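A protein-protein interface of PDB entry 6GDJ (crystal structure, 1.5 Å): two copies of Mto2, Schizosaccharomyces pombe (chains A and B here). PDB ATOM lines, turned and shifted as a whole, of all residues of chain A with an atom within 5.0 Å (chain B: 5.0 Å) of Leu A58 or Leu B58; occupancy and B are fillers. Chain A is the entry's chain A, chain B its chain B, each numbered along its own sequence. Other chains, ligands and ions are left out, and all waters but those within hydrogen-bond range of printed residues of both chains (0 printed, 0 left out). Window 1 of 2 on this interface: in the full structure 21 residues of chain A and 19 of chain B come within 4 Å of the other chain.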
ATOM      1  N   ILE A  25     -12.916  22.424   8.087  1.00  0.00           N
ATOM      2  CA  ILE A  25     -13.088  23.134   9.340  1.00  0.00           C
ATOM      3  C   ILE A  25     -12.753  22.235  10.510  1.00  0.00           C
ATOM      4  O   ILE A  25     -12.057  22.649  11.444  1.00  0.00           O
ATOM      5  CB  ILE A  25     -14.562  23.643   9.529  1.00  0.00           C
ATOM      6  CG1 ILE A  25     -14.956  24.517   8.357  1.00  0.00           C
ATOM      7  CG2 ILE A  25     -14.799  24.349  10.875  1.00  0.00           C
ATOM      8  CD1 ILE A  25     -14.140  25.715   8.283  1.00  0.00           C
ATOM      9  N   PRO A  28      -8.685  21.625  11.429  1.00  0.00           N
ATOM     10  CA  PRO A  28      -7.942  22.646  12.175  1.00  0.00           C
ATOM     11  C   PRO A  28      -8.518  22.875  13.577  1.00  0.00           C
ATOM     12  O   PRO A  28      -7.769  23.174  14.483  1.00  0.00           O
ATOM     13  CB  PRO A  28      -8.064  23.879  11.249  1.00  0.00           C
ATOM     14  CG  PRO A  28      -8.928  23.540  10.168  1.00  0.00           C
ATOM     15  CD  PRO A  28      -9.123  22.087  10.108  1.00  0.00           C
ATOM     16  N   VAL A  29      -9.852  22.775  13.731  1.00  0.00           N
ATOM     17  CA  VAL A  29     -10.423  22.917  15.086  1.00  0.00           C
ATOM     18  C   VAL A  29      -9.896  21.829  15.972  1.00  0.00           C
ATOM     19  O   VAL A  29      -9.473  22.095  17.057  1.00  0.00           O
ATOM     20  CB  VAL A  29     -11.967  22.885  15.047  1.00  0.00           C
ATOM     21  CG1 VAL A  29     -12.481  22.816  16.477  1.00  0.00           C
ATOM     22  CG2 VAL A  29     -12.536  24.104  14.324  1.00  0.00           C
ATOM     23  N   SER A  54     -12.167  30.221  24.660  1.00  0.00           N
ATOM     24  CA  SER A  54     -12.432  30.692  23.330  1.00  0.00           C
ATOM     25  C   SER A  54     -12.652  29.573  22.286  1.00  0.00           C
ATOM     26  O   SER A  54     -13.508  29.693  21.461  1.00  0.00           O
ATOM     27  CB  SER A  54     -11.401  31.656  22.844  1.00  0.00           C
ATOM     28  OG  SER A  54     -10.174  31.061  22.609  1.00  0.00           O
ATOM     29  N   LEU A  55     -11.918  28.464  22.418  1.00  0.00           N
ATOM     30  CA  LEU A  55     -12.156  27.371  21.537  1.00  0.00           C
ATOM     31  C   LEU A  55     -13.433  26.668  21.805  1.00  0.00           C
ATOM     32  O   LEU A  55     -14.120  26.272  20.869  1.00  0.00           O
ATOM     33  CB  LEU A  55     -10.948  26.448  21.595  1.00  0.00           C
ATOM     34  CG  LEU A  55      -9.634  26.964  21.018  1.00  0.00           C
ATOM     35  CD1 LEU A  55      -8.424  26.045  21.286  1.00  0.00           C
ATOM     36  CD2 LEU A  55      -9.795  27.284  19.535  1.00  0.00           C
ATOM     37  N   ALA A  56     -13.819  26.604  23.087  1.00  0.00           N
ATOM     38  CA  ALA A  56     -15.158  26.046  23.410  1.00  0.00           C
ATOM     39  C   ALA A  56     -16.253  26.872  22.742  1.00  0.00           C
ATOM     40  O   ALA A  56     -17.152  26.394  22.106  1.00  0.00           O
ATOM     41  CB  ALA A  56     -15.382  26.039  24.896  1.00  0.00           C
ATOM     42  N   GLU A  57     -16.127  28.197  22.871  1.00  0.00           N
ATOM     43  CA  GLU A  57     -17.097  29.094  22.268  1.00  0.00           C
ATOM     44  C   GLU A  57     -17.155  29.018  20.720  1.00  0.00           C
ATOM     45  O   GLU A  57     -18.207  29.122  20.109  1.00  0.00           O
ATOM     46  CB  GLU A  57     -16.866  30.564  22.737  1.00  0.00           C
ATOM     47  CG  GLU A  57     -16.988  30.822  24.204  1.00  0.00           C
ATOM     48  N   LEU A  58     -15.975  28.809  20.111  1.00  0.00           N
ATOM     49  CA  LEU A  58     -15.931  28.634  18.682  1.00  0.00           C
ATOM     50  C   LEU A  58     -16.728  27.371  18.251  1.00  0.00           C
ATOM     51  O   LEU A  58     -17.531  27.393  17.328  1.00  0.00           O
ATOM     52  CB  LEU A  58     -14.478  28.494  18.253  1.00  0.00           C
ATOM     53  CG  LEU A  58     -14.351  28.133  16.769  1.00  0.00           C
ATOM     54  CD1 LEU A  58     -15.012  29.067  15.815  1.00  0.00           C
ATOM     55  CD2 LEU A  58     -12.896  27.977  16.469  1.00  0.00           C
ATOM     56  N   CYS A  59     -16.467  26.297  18.982  1.00  0.00           N
ATOM     57  CA  CYS A  59     -17.144  25.023  18.705  1.00  0.00           C
ATOM     58  C   CYS A  59     -18.647  25.187  18.860  1.00  0.00           C
ATOM     59  O   CYS A  59     -19.411  24.705  18.051  1.00  0.00           O
ATOM     60  CB  CYS A  59     -16.623  23.933  19.631  1.00  0.00           C
ATOM     61  SG  CYS A  59     -14.973  23.326  19.210  1.00  0.00           S
ATOM     62  N   LEU A  60     -19.048  25.890  19.911  1.00  0.00           N
ATOM     63  CA  LEU A  60     -20.487  26.108  20.124  1.00  0.00           C
ATOM     64  C   LEU A  60     -21.140  27.026  19.083  1.00  0.00           C
ATOM     65  O   LEU A  60     -22.278  26.882  18.682  1.00  0.00           O
ATOM     66  CB  LEU A  60     -20.738  26.615  21.537  1.00  0.00           C
ATOM     67  CG  LEU A  60     -20.394  25.633  22.681  1.00  0.00           C
ATOM     68  CD1 LEU A  60     -20.706  26.291  24.030  1.00  0.00           C
ATOM     69  CD2 LEU A  60     -21.066  24.292  22.436  1.00  0.00           C
ATOM     70  N   GLY A  61     -20.349  27.986  18.551  1.00  0.00           N
ATOM     71  CA  GLY A  61     -20.868  28.831  17.509  1.00  0.00           C
ATOM     72  C   GLY A  61     -21.016  28.077  16.221  1.00  0.00           C
ATOM     73  O   GLY A  61     -21.990  28.250  15.522  1.00  0.00           O
ATOM     74  N   LEU A  62     -20.049  27.152  15.956  1.00  0.00           N
ATOM     75  CA  LEU A  62     -20.190  26.254  14.792  1.00  0.00           C
ATOM     76  C   LEU A  62     -21.380  25.283  14.911  1.00  0.00           C
ATOM     77  O   LEU A  62     -22.117  25.067  13.966  1.00  0.00           O
ATOM     78  CB  LEU A  62     -18.889  25.466  14.551  1.00  0.00           C
ATOM     79  CG  LEU A  62     -17.699  26.325  14.118  1.00  0.00           C
ATOM     80  CD1 LEU A  62     -16.436  25.539  14.277  1.00  0.00           C
ATOM     81  CD2 LEU A  62     -17.906  26.804  12.679  1.00  0.00           C
ATOM     82  N   VAL A  63     -21.641  24.855  16.138  1.00  0.00           N
ATOM     83  CA  VAL A  63     -22.853  24.053  16.420  1.00  0.00           C
ATOM     84  C   VAL A  63     -24.122  24.870  16.137  1.00  0.00           C
ATOM     85  O   VAL A  63     -25.019  24.419  15.472  1.00  0.00           O
ATOM     86  CB  VAL A  63     -22.860  23.539  17.893  1.00  0.00           C
ATOM     87  CG1 VAL A  63     -24.257  23.106  18.323  1.00  0.00           C
ATOM     88  CG2 VAL A  63     -21.835  22.445  18.100  1.00  0.00           C
ATOM     89  N   ILE B  25     -19.296  33.030  15.076  1.00  0.00           N
ATOM     90  CA  ILE B  25     -18.065  32.347  14.734  1.00  0.00           C
ATOM     91  C   ILE B  25     -16.857  33.293  14.839  1.00  0.00           C
ATOM     92  O   ILE B  25     -15.834  32.953  15.409  1.00  0.00           O
ATOM     93  CB  ILE B  25     -18.118  31.859  13.213  1.00  0.00           C
ATOM     94  CG1 ILE B  25     -19.279  30.940  12.976  1.00  0.00           C
ATOM     95  CG2 ILE B  25     -16.781  31.259  12.742  1.00  0.00           C
ATOM     96  CD1 ILE B  25     -19.287  29.936  13.994  1.00  0.00           C
ATOM     97  N   PRO B  28     -15.375  34.381  18.633  1.00  0.00           N
ATOM     98  CA  PRO B  28     -14.421  33.457  19.302  1.00  0.00           C
ATOM     99  C   PRO B  28     -13.124  33.191  18.571  1.00  0.00           C
ATOM    100  O   PRO B  28     -12.116  32.962  19.218  1.00  0.00           O
ATOM    101  CB  PRO B  28     -15.260  32.163  19.524  1.00  0.00           C
ATOM    102  CG  PRO B  28     -16.502  32.348  18.818  1.00  0.00           C
ATOM    103  CD  PRO B  28     -16.707  33.774  18.433  1.00  0.00           C
ATOM    104  N   VAL B  29     -13.185  33.260  17.227  1.00  0.00           N
ATOM    105  CA  VAL B  29     -11.925  33.111  16.459  1.00  0.00           C
ATOM    106  C   VAL B  29     -10.973  34.261  16.837  1.00  0.00           C
ATOM    107  O   VAL B  29      -9.805  34.071  17.105  1.00  0.00           O
ATOM    108  CB  VAL B  29     -12.179  33.083  14.967  1.00  0.00           C
ATOM    109  CG1 VAL B  29     -10.857  33.246  14.227  1.00  0.00           C
ATOM    110  CG2 VAL B  29     -12.940  31.816  14.603  1.00  0.00           C
ATOM    111  N   SER B  54      -2.441  26.083  13.368  1.00  0.00           N
ATOM    112  CA  SER B  54      -3.788  25.515  13.363  1.00  0.00           C
ATOM    113  C   SER B  54      -4.880  26.578  13.228  1.00  0.00           C
ATOM    114  O   SER B  54      -5.865  26.429  12.514  1.00  0.00           O
ATOM    115  CB  SER B  54      -4.087  24.696  14.650  1.00  0.00           C
ATOM    116  OG  SER B  54      -3.185  23.553  14.605  1.00  0.00           O
ATOM    117  N   LEU B  55      -4.644  27.720  13.903  1.00  0.00           N
ATOM    118  CA  LEU B  55      -5.608  28.818  13.791  1.00  0.00           C
ATOM    119  C   LEU B  55      -5.570  29.477  12.452  1.00  0.00           C
ATOM    120  O   LEU B  55      -6.602  29.829  11.913  1.00  0.00           O
ATOM    121  CB  LEU B  55      -5.424  29.829  14.920  1.00  0.00           C
ATOM    122  CG  LEU B  55      -5.685  29.335  16.332  1.00  0.00           C
ATOM    123  CD1 LEU B  55      -5.277  30.307  17.375  1.00  0.00           C
ATOM    124  CD2 LEU B  55      -7.184  28.935  16.513  1.00  0.00           C
ATOM    125  N   ALA B  56      -4.389  29.544  11.829  1.00  0.00           N
ATOM    126  CA  ALA B  56      -4.320  30.009  10.436  1.00  0.00           C
ATOM    127  C   ALA B  56      -5.112  29.110   9.494  1.00  0.00           C
ATOM    128  O   ALA B  56      -5.916  29.547   8.713  1.00  0.00           O
ATOM    129  CB  ALA B  56      -2.910  30.046   9.995  1.00  0.00           C
ATOM    130  N   GLU B  57      -4.901  27.794   9.690  1.00  0.00           N
ATOM    131  CA  GLU B  57      -5.607  26.812   8.860  1.00  0.00           C
ATOM    132  C   GLU B  57      -7.106  26.863   9.061  1.00  0.00           C
ATOM    133  O   GLU B  57      -7.872  26.661   8.153  1.00  0.00           O
ATOM    134  CB  GLU B  57      -5.100  25.410   9.196  1.00  0.00           C
ATOM    135  CG  GLU B  57      -5.546  24.329   8.281  1.00  0.00           C
ATOM    136  CD  GLU B  57      -5.160  22.977   8.835  1.00  0.00           C
ATOM    137  OE1 GLU B  57      -4.253  22.901   9.771  1.00  0.00           O
ATOM    138  OE2 GLU B  57      -5.850  21.973   8.465  1.00  0.00           O
ATOM    139  N   LEU B  58      -7.538  27.122  10.318  1.00  0.00           N
ATOM    140  CA  LEU B  58      -8.959  27.301  10.588  1.00  0.00           C
ATOM    141  C   LEU B  58      -9.521  28.450   9.817  1.00  0.00           C
ATOM    142  O   LEU B  58     -10.550  28.357   9.191  1.00  0.00           O
ATOM    143  CB  LEU B  58      -9.164  27.489  12.113  1.00  0.00           C
ATOM    144  CG  LEU B  58     -10.609  27.915  12.440  1.00  0.00           C
ATOM    145  CD1 LEU B  58     -11.654  26.893  12.052  1.00  0.00           C
ATOM    146  CD2 LEU B  58     -10.640  28.253  13.906  1.00  0.00           C
ATOM    147  N   CYS B  59      -8.846  29.595   9.896  1.00  0.00           N
ATOM    148  CA  CYS B  59      -9.318  30.756   9.202  1.00  0.00           C
ATOM    149  C   CYS B  59      -9.405  30.554   7.674  1.00  0.00           C
ATOM    150  O   CYS B  59     -10.352  30.935   7.047  1.00  0.00           O
ATOM    151  CB  CYS B  59      -8.404  31.975   9.514  1.00  0.00           C
ATOM    152  SG  CYS B  59      -8.618  32.576  11.205  1.00  0.00           S
ATOM    153  N   LEU B  60      -8.411  29.867   7.121  1.00  0.00           N
ATOM    154  CA  LEU B  60      -8.394  29.572   5.683  1.00  0.00           C
ATOM    155  C   LEU B  60      -9.432  28.560   5.274  1.00  0.00           C
ATOM    156  O   LEU B  60     -10.030  28.689   4.202  1.00  0.00           O
ATOM    157  CB  LEU B  60      -6.990  29.137   5.292  1.00  0.00           C
ATOM    158  CG  LEU B  60      -5.850  30.116   5.443  1.00  0.00           C
ATOM    159  CD1 LEU B  60      -4.512  29.555   5.032  1.00  0.00           C
ATOM    160  CD2 LEU B  60      -6.237  31.371   4.665  1.00  0.00           C
ATOM    161  N   GLY B  61      -9.766  27.647   6.201  1.00  0.00           N
ATOM    162  CA  GLY B  61     -10.869  26.779   6.003  1.00  0.00           C
ATOM    163  C   GLY B  61     -12.215  27.458   6.002  1.00  0.00           C
ATOM    164  O   GLY B  61     -13.112  27.187   5.190  1.00  0.00           O
ATOM    165  N   LEU B  62     -12.370  28.411   6.942  1.00  0.00           N
ATOM    166  CA  LEU B  62     -13.579  29.217   6.967  1.00  0.00           C
ATOM    167  C   LEU B  62     -13.743  30.099   5.714  1.00  0.00           C
ATOM    168  O   LEU B  62     -14.853  30.290   5.203  1.00  0.00           O
ATOM    169  CB  LEU B  62     -13.656  30.088   8.240  1.00  0.00           C
ATOM    170  CG  LEU B  62     -13.867  29.265   9.501  1.00  0.00           C
ATOM    171  CD1 LEU B  62     -13.525  30.063  10.709  1.00  0.00           C
ATOM    172  CD2 LEU B  62     -15.303  28.744   9.578  1.00  0.00           C
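Leu B58 touches just these residues of chain A: Pro A28 (3.4 Å), Val A29 (3.7 Å) and Leu A58 (3.4 Å).
Printed residues of chain A within 4 Å of Gly B61: Ile A25 (3.5 Å).
Of the printed residues of chain A, Ser B54 touches Pro A28.
Printed residues of chain A within 4 Å of Leu B62: Ile A25 (3.5 Å).
Of the printed residues of chain A, Glu B57 touches Pro A28.
Printed residues of chain B within 4 Å of Gly A61: Ile B25.
Ala B56 touches none of the printed residues of chain A.
Cys A59 touches none of the printed residues of chain B.
The nearest printed residue of chain B that does not touch Leu A58 is Leu B62 (5.4 Å).
The nearest residue of chain A that does not touch Leu B58 is Ile A25 (4.2 Å).
Of the 13 printed residues of chain A, 8 touch a printed residue of chain B.
Printed residues of chain A that touch a printed residue of chain B: Ile A25, Pro A28, Val A29, Ser A54, Glu A57, Leu A58, Gly A61 and Leu A62.
Hydrophobic or aromatic side chains of chain A that line the printed part of chain B: Ile A25, Pro A28, Val A29, Leu A58 and Leu A62.
Among the printed residues, 14 pairs touch across the chains.
Ile A25 touches Gly B61, and with the chains exchanged Gly A61 touches Ile B25.
Pro A28 touches Leu B58, and with the chains exchanged Leu A58 touches Pro B28.
Val A29 touches Leu B58, and with the chains exchanged Leu A58 touches Val B29.
Leu A58 touches Ile B25, but with the chains exchanged Ile A25 does not touch Leu B58 (4.2 Å).
Positions printed for both chains: 25, 28, 29, 54, 55, 56, 57, 58, 59, 60, 61 and 62.
Of the 14 pairs that touch across the chains among the printed residues, 13 have their exchanged pair printed and touching as well.
CD1 of Ile A25 touches N of Leu B62 (3.5 Å).
O of Ser B54 touches CB of Pro A28 (3.6 Å).
Pro A28 touches Glu B57 (CD to OE2, 3.7 Å).
Leu B58 touches Val A29.
Ser A54 touches Pro B28.
CB of Pro B28 touches C of Glu A57, 3.9 Å away.
Leu A58 touches Ile B25.
CB of Pro B28 touches N of Leu A58 (3.5 Å).
Leu A58 touches Leu B58.
Gly A61 touches Ile B25.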
